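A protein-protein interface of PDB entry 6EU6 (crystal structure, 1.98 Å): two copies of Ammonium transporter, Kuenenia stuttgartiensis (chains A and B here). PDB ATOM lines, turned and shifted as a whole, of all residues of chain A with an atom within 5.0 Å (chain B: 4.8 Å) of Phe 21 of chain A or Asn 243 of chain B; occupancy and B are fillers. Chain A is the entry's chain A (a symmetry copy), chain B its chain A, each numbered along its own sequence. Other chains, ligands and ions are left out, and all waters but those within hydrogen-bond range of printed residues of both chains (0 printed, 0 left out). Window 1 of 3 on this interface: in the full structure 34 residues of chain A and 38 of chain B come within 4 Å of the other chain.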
ATOM      1  N   ALA A  17       8.390  18.661 -19.901  1.00  0.00           N
ATOM      2  CA  ALA A  17       7.818  18.619 -21.213  1.00  0.00           C
ATOM      3  C   ALA A  17       6.601  17.665 -21.268  1.00  0.00           C
ATOM      4  O   ALA A  17       5.573  17.927 -21.931  1.00  0.00           O
ATOM      5  CB  ALA A  17       8.853  18.226 -22.247  1.00  0.00           C
ATOM      6  N   CYS A  18       6.733  16.555 -20.612  1.00  0.00           N
ATOM      7  CA  CYS A  18       5.647  15.610 -20.555  1.00  0.00           C
ATOM      8  C   CYS A  18       4.451  16.233 -19.798  1.00  0.00           C
ATOM      9  O   CYS A  18       3.291  16.004 -20.159  1.00  0.00           O
ATOM     10  CB  CYS A  18       6.059  14.314 -19.866  1.00  0.00           C
ATOM     11  SG  CYS A  18       7.304  13.370 -20.769  1.00  0.00           S
ATOM     12  N   MET A  19       4.716  17.018 -18.760  1.00  0.00           N
ATOM     13  CA  MET A  19       3.605  17.670 -18.057  1.00  0.00           C
ATOM     14  C   MET A  19       2.896  18.654 -19.000  1.00  0.00           C
ATOM     15  O   MET A  19       1.669  18.814 -18.992  1.00  0.00           O
ATOM     16  CB  MET A  19       4.107  18.394 -16.793  1.00  0.00           C
ATOM     17  CG  MET A  19       4.702  17.505 -15.766  1.00  0.00           C
ATOM     18  SD  MET A  19       5.581  18.308 -14.436  1.00  0.00           S
ATOM     19  CE  MET A  19       4.220  19.158 -13.592  1.00  0.00           C
ATOM     20  N   VAL A  20       3.678  19.385 -19.765  1.00  0.00           N
ATOM     21  CA  VAL A  20       3.111  20.293 -20.781  1.00  0.00           C
ATOM     22  C   VAL A  20       2.361  19.570 -21.889  1.00  0.00           C
ATOM     23  O   VAL A  20       1.291  20.008 -22.364  1.00  0.00           O
ATOM     24  CB  VAL A  20       4.225  21.174 -21.403  1.00  0.00           C
ATOM     25  CG1 VAL A  20       3.656  22.035 -22.536  1.00  0.00           C
ATOM     26  CG2 VAL A  20       4.840  22.066 -20.304  1.00  0.00           C
ATOM     27  N   PHE A  21       2.830  18.371 -22.262  1.00  0.00           N
ATOM     28  CA  PHE A  21       2.036  17.569 -23.200  1.00  0.00           C
ATOM     29  C   PHE A  21       0.621  17.320 -22.642  1.00  0.00           C
ATOM     30  O   PHE A  21      -0.382  17.332 -23.344  1.00  0.00           O
ATOM     31  CB  PHE A  21       2.731  16.207 -23.503  1.00  0.00           C
ATOM     32  CG  PHE A  21       1.942  15.360 -24.412  1.00  0.00           C
ATOM     33  CD1 PHE A  21       2.060  15.497 -25.795  1.00  0.00           C
ATOM     34  CD2 PHE A  21       1.064  14.435 -23.907  1.00  0.00           C
ATOM     35  CE1 PHE A  21       1.325  14.658 -26.647  1.00  0.00           C
ATOM     36  CE2 PHE A  21       0.303  13.632 -24.760  1.00  0.00           C
ATOM     37  CZ  PHE A  21       0.419  13.761 -26.127  1.00  0.00           C
ATOM     38  N   LEU A  22       0.573  17.043 -21.355  1.00  0.00           N
ATOM     39  CA  LEU A  22      -0.694  16.747 -20.702  1.00  0.00           C
ATOM     40  C   LEU A  22      -1.673  17.956 -20.666  1.00  0.00           C
ATOM     41  O   LEU A  22      -2.887  17.744 -20.607  1.00  0.00           O
ATOM     42  CB  LEU A  22      -0.440  16.286 -19.261  1.00  0.00           C
ATOM     43  CG  LEU A  22      -1.551  15.459 -18.642  1.00  0.00           C
ATOM     44  CD1 LEU A  22      -1.753  14.187 -19.413  1.00  0.00           C
ATOM     45  CD2 LEU A  22      -1.178  15.137 -17.205  1.00  0.00           C
ATOM     46  N   MET A  23      -1.149  19.165 -20.841  1.00  0.00           N
ATOM     47  CA  MET A  23      -1.995  20.328 -21.093  1.00  0.00           C
ATOM     48  C   MET A  23      -2.816  20.157 -22.332  1.00  0.00           C
ATOM     49  O   MET A  23      -3.867  20.707 -22.427  1.00  0.00           O
ATOM     50  CB  MET A  23      -1.164  21.598 -21.181  1.00  0.00           C
ATOM     51  CG  MET A  23      -0.519  21.943 -19.873  1.00  0.00           C
ATOM     52  SD  MET A  23       0.570  23.381 -20.024  1.00  0.00           S
ATOM     53  CE  MET A  23      -0.555  24.769 -20.124  1.00  0.00           C
ATOM     54  N   GLN A  24      -2.342  19.399 -23.305  1.00  0.00           N
ATOM     55  CA  GLN A  24      -3.137  19.166 -24.516  1.00  0.00           C
ATOM     56  C   GLN A  24      -4.487  18.487 -24.158  1.00  0.00           C
ATOM     57  O   GLN A  24      -5.557  18.708 -24.782  1.00  0.00           O
ATOM     58  CB  GLN A  24      -2.361  18.301 -25.515  1.00  0.00           C
ATOM     59  CG  GLN A  24      -1.123  18.968 -26.068  1.00  0.00           C
ATOM     60  CD  GLN A  24      -1.472  20.072 -27.074  1.00  0.00           C
ATOM     61  OE1 GLN A  24      -2.070  19.839 -28.153  1.00  0.00           O
ATOM     62  NE2 GLN A  24      -1.190  21.264 -26.696  1.00  0.00           N
ATOM     63  N   LEU A  25      -4.393  17.570 -23.223  1.00  0.00           N
ATOM     64  CA  LEU A  25      -5.591  16.941 -22.619  1.00  0.00           C
ATOM     65  C   LEU A  25      -6.423  17.958 -21.828  1.00  0.00           C
ATOM     66  O   LEU A  25      -7.661  17.987 -21.944  1.00  0.00           O
ATOM     67  CB  LEU A  25      -5.114  15.790 -21.738  1.00  0.00           C
ATOM     68  CG  LEU A  25      -6.143  14.778 -21.212  1.00  0.00           C
ATOM     69  CD1 LEU A  25      -5.410  13.592 -20.619  1.00  0.00           C
ATOM     70  CD2 LEU A  25      -7.013  15.357 -20.153  1.00  0.00           C
ATOM     71  N   THR A  51      -2.593  18.253 -32.187  1.00  0.00           N
ATOM     72  CA  THR A  51      -1.381  17.798 -31.589  1.00  0.00           C
ATOM     73  C   THR A  51      -0.545  17.015 -32.649  1.00  0.00           C
ATOM     74  O   THR A  51       0.696  17.127 -32.707  1.00  0.00           O
ATOM     75  CB  THR A  51      -1.733  16.906 -30.381  1.00  0.00           C
ATOM     76  OG1 THR A  51      -2.526  17.645 -29.438  1.00  0.00           O
ATOM     77  CG2 THR A  51      -0.489  16.439 -29.743  1.00  0.00           C
ATOM     78  N   SER A  55       3.110  18.737 -33.961  1.00  0.00           N
ATOM     79  CA  SER A  55       4.339  17.971 -33.720  1.00  0.00           C
ATOM     80  C   SER A  55       5.119  17.860 -35.023  1.00  0.00           C
ATOM     81  O   SER A  55       6.313  18.031 -35.040  1.00  0.00           O
ATOM     82  CB  SER A  55       4.036  16.553 -33.256  1.00  0.00           C
ATOM     83  OG  SER A  55       3.463  16.483 -31.940  1.00  0.00           O
ATOM     84  N   PHE A  98      12.118  18.696 -27.519  1.00  0.00           N
ATOM     85  CA  PHE A  98      10.790  18.214 -27.264  1.00  0.00           C
ATOM     86  C   PHE A  98      10.009  19.205 -26.412  1.00  0.00           C
ATOM     87  O   PHE A  98       8.807  19.400 -26.636  1.00  0.00           O
ATOM     88  CB  PHE A  98      10.822  16.832 -26.598  1.00  0.00           C
ATOM     89  CG  PHE A  98       9.446  16.245 -26.396  1.00  0.00           C
ATOM     90  CD1 PHE A  98       8.550  16.112 -27.465  1.00  0.00           C
ATOM     91  CD2 PHE A  98       8.994  15.941 -25.133  1.00  0.00           C
ATOM     92  CE1 PHE A  98       7.251  15.664 -27.281  1.00  0.00           C
ATOM     93  CE2 PHE A  98       7.693  15.471 -24.942  1.00  0.00           C
ATOM     94  CZ  PHE A  98       6.829  15.320 -26.013  1.00  0.00           C
ATOM     95  N   MET A 101       8.827  21.715 -28.627  1.00  0.00           N
ATOM     96  CA  MET A 101       7.735  21.218 -29.440  1.00  0.00           C
ATOM     97  C   MET A 101       6.395  21.315 -28.710  1.00  0.00           C
ATOM     98  O   MET A 101       5.389  21.713 -29.288  1.00  0.00           O
ATOM     99  CB  MET A 101       7.993  19.752 -29.884  1.00  0.00           C
ATOM    100  CG  MET A 101       6.902  19.160 -30.748  1.00  0.00           C
ATOM    101  SD  MET A 101       7.317  17.446 -31.219  1.00  0.00           S
ATOM    102  CE  MET A 101       8.531  17.889 -32.447  1.00  0.00           C
ATOM    103  N   VAL A 102       6.374  20.895 -27.441  1.00  0.00           N
ATOM    104  CA  VAL A 102       5.109  20.950 -26.740  1.00  0.00           C
ATOM    105  C   VAL A 102       4.689  22.424 -26.455  1.00  0.00           C
ATOM    106  O   VAL A 102       3.508  22.721 -26.352  1.00  0.00           O
ATOM    107  CB  VAL A 102       5.074  20.042 -25.486  1.00  0.00           C
ATOM    108  CG1 VAL A 102       5.262  18.581 -25.912  1.00  0.00           C
ATOM    109  CG2 VAL A 102       6.108  20.404 -24.454  1.00  0.00           C
ATOM    110  N   PHE B 214      -4.883  10.520 -25.048  1.00  0.00           N
ATOM    111  CA  PHE B 214      -3.876  11.406 -24.477  1.00  0.00           C
ATOM    112  C   PHE B 214      -3.177  10.854 -23.243  1.00  0.00           C
ATOM    113  O   PHE B 214      -1.954  10.995 -23.076  1.00  0.00           O
ATOM    114  CB  PHE B 214      -4.453  12.776 -24.174  1.00  0.00           C
ATOM    115  CG  PHE B 214      -4.518  13.717 -25.344  1.00  0.00           C
ATOM    116  CD1 PHE B 214      -3.360  14.203 -25.962  1.00  0.00           C
ATOM    117  CD2 PHE B 214      -5.760  14.211 -25.768  1.00  0.00           C
ATOM    118  CE1 PHE B 214      -3.466  15.139 -27.033  1.00  0.00           C
ATOM    119  CE2 PHE B 214      -5.840  15.152 -26.833  1.00  0.00           C
ATOM    120  CZ  PHE B 214      -4.672  15.612 -27.399  1.00  0.00           C
ATOM    121  N   TRP B 217      -0.810   8.090 -24.381  1.00  0.00           N
ATOM    122  CA  TRP B 217       0.358   8.688 -25.083  1.00  0.00           C
ATOM    123  C   TRP B 217       1.363   9.272 -24.033  1.00  0.00           C
ATOM    124  O   TRP B 217       2.593   9.022 -24.046  1.00  0.00           O
ATOM    125  CB  TRP B 217      -0.196   9.709 -26.058  1.00  0.00           C
ATOM    126  CG  TRP B 217       0.734  10.483 -27.003  1.00  0.00           C
ATOM    127  CD1 TRP B 217       2.053  10.736 -26.855  1.00  0.00           C
ATOM    128  CD2 TRP B 217       0.340  11.102 -28.220  1.00  0.00           C
ATOM    129  NE1 TRP B 217       2.502  11.556 -27.896  1.00  0.00           N
ATOM    130  CE2 TRP B 217       1.468  11.769 -28.751  1.00  0.00           C
ATOM    131  CE3 TRP B 217      -0.864  11.207 -28.874  1.00  0.00           C
ATOM    132  CZ2 TRP B 217       1.428  12.499 -29.921  1.00  0.00           C
ATOM    133  CZ3 TRP B 217      -0.921  11.940 -30.046  1.00  0.00           C
ATOM    134  CH2 TRP B 217       0.234  12.568 -30.568  1.00  0.00           C
ATOM    135  N   PHE B 218       0.829  10.050 -23.097  1.00  0.00           N
ATOM    136  CA  PHE B 218       1.594  10.556 -21.972  1.00  0.00           C
ATOM    137  C   PHE B 218       2.268   9.452 -21.213  1.00  0.00           C
ATOM    138  O   PHE B 218       3.450   9.484 -21.015  1.00  0.00           O
ATOM    139  CB  PHE B 218       0.671  11.283 -21.025  1.00  0.00           C
ATOM    140  CG  PHE B 218       1.309  11.694 -19.772  1.00  0.00           C
ATOM    141  CD1 PHE B 218       2.000  12.907 -19.694  1.00  0.00           C
ATOM    142  CD2 PHE B 218       1.152  10.946 -18.645  1.00  0.00           C
ATOM    143  CE1 PHE B 218       2.560  13.322 -18.502  1.00  0.00           C
ATOM    144  CE2 PHE B 218       1.758  11.305 -17.436  1.00  0.00           C
ATOM    145  CZ  PHE B 218       2.466  12.507 -17.361  1.00  0.00           C
ATOM    146  N   PHE B 221       5.386   7.849 -22.742  1.00  0.00           N
ATOM    147  CA  PHE B 221       6.628   8.542 -22.490  1.00  0.00           C
ATOM    148  C   PHE B 221       7.446   7.909 -21.371  1.00  0.00           C
ATOM    149  O   PHE B 221       8.714   7.741 -21.498  1.00  0.00           O
ATOM    150  CB  PHE B 221       6.428  10.053 -22.196  1.00  0.00           C
ATOM    151  CG  PHE B 221       5.881  10.860 -23.366  1.00  0.00           C
ATOM    152  CD1 PHE B 221       6.211  10.555 -24.690  1.00  0.00           C
ATOM    153  CD2 PHE B 221       5.007  11.910 -23.142  1.00  0.00           C
ATOM    154  CE1 PHE B 221       5.696  11.309 -25.730  1.00  0.00           C
ATOM    155  CE2 PHE B 221       4.473  12.639 -24.195  1.00  0.00           C
ATOM    156  CZ  PHE B 221       4.844  12.335 -25.479  1.00  0.00           C
ATOM    157  N   ILE B 239      11.947   9.852 -25.837  1.00  0.00           N
ATOM    158  CA  ILE B 239      10.613  10.503 -25.721  1.00  0.00           C
ATOM    159  C   ILE B 239      10.194  11.229 -26.987  1.00  0.00           C
ATOM    160  O   ILE B 239       9.050  11.156 -27.385  1.00  0.00           O
ATOM    161  CB  ILE B 239      10.620  11.374 -24.475  1.00  0.00           C
ATOM    162  CG1 ILE B 239      10.554  10.385 -23.308  1.00  0.00           C
ATOM    163  CG2 ILE B 239       9.433  12.328 -24.468  1.00  0.00           C
ATOM    164  CD1 ILE B 239      10.527  10.899 -21.917  1.00  0.00           C
ATOM    165  N   LEU B 240      11.133  11.935 -27.601  1.00  0.00           N
ATOM    166  CA  LEU B 240      10.893  12.569 -28.884  1.00  0.00           C
ATOM    167  C   LEU B 240      10.519  11.536 -29.935  1.00  0.00           C
ATOM    168  O   LEU B 240       9.516  11.681 -30.625  1.00  0.00           O
ATOM    169  CB  LEU B 240      12.123  13.372 -29.322  1.00  0.00           C
ATOM    170  CG  LEU B 240      11.969  14.031 -30.711  1.00  0.00           C
ATOM    171  CD1 LEU B 240      10.806  15.065 -30.723  1.00  0.00           C
ATOM    172  CD2 LEU B 240      13.250  14.689 -31.223  1.00  0.00           C
ATOM    173  N   ASN B 241      11.233  10.404 -29.987  1.00  0.00           N
ATOM    174  CA  ASN B 241      10.839   9.402 -30.938  1.00  0.00           C
ATOM    175  C   ASN B 241       9.461   8.844 -30.631  1.00  0.00           C
ATOM    176  O   ASN B 241       8.692   8.524 -31.552  1.00  0.00           O
ATOM    177  CB  ASN B 241      11.832   8.228 -30.955  1.00  0.00           C
ATOM    178  CG  ASN B 241      13.149   8.579 -31.575  1.00  0.00           C
ATOM    179  OD1 ASN B 241      13.292   9.559 -32.345  1.00  0.00           O
ATOM    180  ND2 ASN B 241      14.164   7.778 -31.224  1.00  0.00           N
ATOM    181  N   THR B 242       9.134   8.634 -29.343  1.00  0.00           N
ATOM    182  CA  THR B 242       7.827   8.127 -29.030  1.00  0.00           C
ATOM    183  C   THR B 242       6.747   9.096 -29.560  1.00  0.00           C
ATOM    184  O   THR B 242       5.804   8.703 -30.151  1.00  0.00           O
ATOM    185  CB  THR B 242       7.733   7.942 -27.501  1.00  0.00           C
ATOM    186  OG1 THR B 242       8.721   6.973 -27.124  1.00  0.00           O
ATOM    187  CG2 THR B 242       6.370   7.478 -27.087  1.00  0.00           C
ATOM    188  N   ASN B 243       6.958  10.398 -29.362  1.00  0.00           N
ATOM    189  CA  ASN B 243       6.013  11.398 -29.770  1.00  0.00           C
ATOM    190  C   ASN B 243       5.867  11.427 -31.283  1.00  0.00           C
ATOM    191  O   ASN B 243       4.747  11.532 -31.863  1.00  0.00           O
ATOM    192  CB  ASN B 243       6.411  12.770 -29.297  1.00  0.00           C
ATOM    193  CG  ASN B 243       5.271  13.738 -29.439  1.00  0.00           C
ATOM    194  OD1 ASN B 243       4.305  13.692 -28.683  1.00  0.00           O
ATOM    195  ND2 ASN B 243       5.383  14.653 -30.418  1.00  0.00           N
ATOM    196  N   MET B 244       7.000  11.338 -31.939  1.00  0.00           N
ATOM    197  CA  MET B 244       6.955  11.439 -33.379  1.00  0.00           C
ATOM    198  C   MET B 244       6.286  10.223 -34.005  1.00  0.00           C
ATOM    199  O   MET B 244       5.637  10.373 -35.034  1.00  0.00           O
ATOM    200  CB  MET B 244       8.373  11.651 -33.990  1.00  0.00           C
ATOM    201  CG  MET B 244       9.074  12.884 -33.499  1.00  0.00           C
ATOM    202  SD  MET B 244       8.099  14.351 -33.739  1.00  0.00           S
ATOM    203  CE  MET B 244       7.825  14.385 -35.523  1.00  0.00           C
ATOM    204  N   ALA B 245       6.454   9.019 -33.434  1.00  0.00           N
ATOM    205  CA  ALA B 245       5.794   7.840 -33.983  1.00  0.00           C
ATOM    206  C   ALA B 245       4.273   8.023 -33.857  1.00  0.00           C
ATOM    207  O   ALA B 245       3.551   7.735 -34.827  1.00  0.00           O
ATOM    208  CB  ALA B 245       6.223   6.510 -33.334  1.00  0.00           C
ATOM    209  N   ALA B 246       3.775   8.456 -32.679  1.00  0.00           N
ATOM    210  CA  ALA B 246       2.345   8.690 -32.470  1.00  0.00           C
ATOM    211  C   ALA B 246       1.813   9.733 -33.464  1.00  0.00           C
ATOM    212  O   ALA B 246       0.756   9.545 -34.125  1.00  0.00           O
ATOM    213  CB  ALA B 246       2.048   9.144 -31.063  1.00  0.00           C
ATOM    214  N   ALA B 247       2.539  10.821 -33.584  1.00  0.00           N
ATOM    215  CA  ALA B 247       2.041  11.918 -34.414  1.00  0.00           C
ATOM    216  C   ALA B 247       2.011  11.487 -35.897  1.00  0.00           C
ATOM    217  O   ALA B 247       1.033  11.707 -36.588  1.00  0.00           O
ATOM    218  CB  ALA B 247       2.939  13.095 -34.252  1.00  0.00           C
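ND2 of Asn 243 of chain B sits at hydrogen-bond distance from OG of Ser 55 of chain A (3.1 Å). The side-chain sulfur (SD) of Met 101 of chain A sits at hydrogen-bond distance from the side-chain amide nitrogen (ND2) of Asn 243 of chain B (3.5 Å).
The side-chain amide oxygen (OD1) of Asn 243 of chain B is in hydrogen-bond range of the indole nitrogen (NE1) of Trp 217 of chain B. OG of Ser 55 of chain A is in hydrogen-bond range of O of Thr 51 of chain A. OE1 of Gln 24 of chain A lies within hydrogen-bond range of OG1 of Thr 51 of chain A (2.6 Å).
Among the printed residues, pairs that only touch across the chains: Cys 18 of chain A with Phe 218 of chain B, Cys 18 of chain A with Phe 221 of chain B, Phe 21 of chain A with Phe 214 of chain B, Phe 21 of chain A with Trp 217 of chain B, Phe 21 of chain A with Phe 218 of chain B, Phe 21 of chain A with Phe 221 of chain B, Phe 21 of chain A with Asn 243 of chain B, Leu 22 of chain A with Phe 218 of chain B, Gln 24 of chain A with Phe 214 of chain B, Leu 25 of chain A with Phe 214 of chain B, Thr 51 of chain A with Phe 214 of chain B, Ser 55 of chain A with Met 244 of chain B, Ser 55 of chain A with Ala 247 of chain B, Phe 98 of chain A with Phe 221 of chain B, Phe 98 of chain A with Ile 239 of chain B, Phe 98 of chain A with Asn 243 of chain B and Met 101 of chain A with Met 244 of chain B.
Of the printed residues of chain B, Phe 21 of chain A touches Phe 214 (3.8 Å), Trp 217 (3.4 Å), Phe 218 (3.98 Å), Phe 221 (3.7 Å) and Asn 243 (3.7 Å). Printed residues of chain B within 4 Å of Phe 98 of chain A: Phe 221 (3.6 Å), Ile 239 (3.6 Å) and Asn 243 (3.5 Å). Of the printed residues of chain A, Ile 239 of chain B touches Phe 98. Asn 243 of chain B touches four residues of chain A. The nearest printed residue of chain B that does not touch Phe 21 of chain A is Ala 246 of chain B (7.0 Å). The nearest printed residue of chain A that does not touch Asn 243 of chain B is Thr 51 of chain A (5.6 Å). The nearest printed residue of chain A that does not touch Phe 214 of chain B is Leu 22 of chain A (4.9 Å).
Along chain B the printed residues that touch a printed residue of chain A span positions 214 to 247.
No position is printed for both chains.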
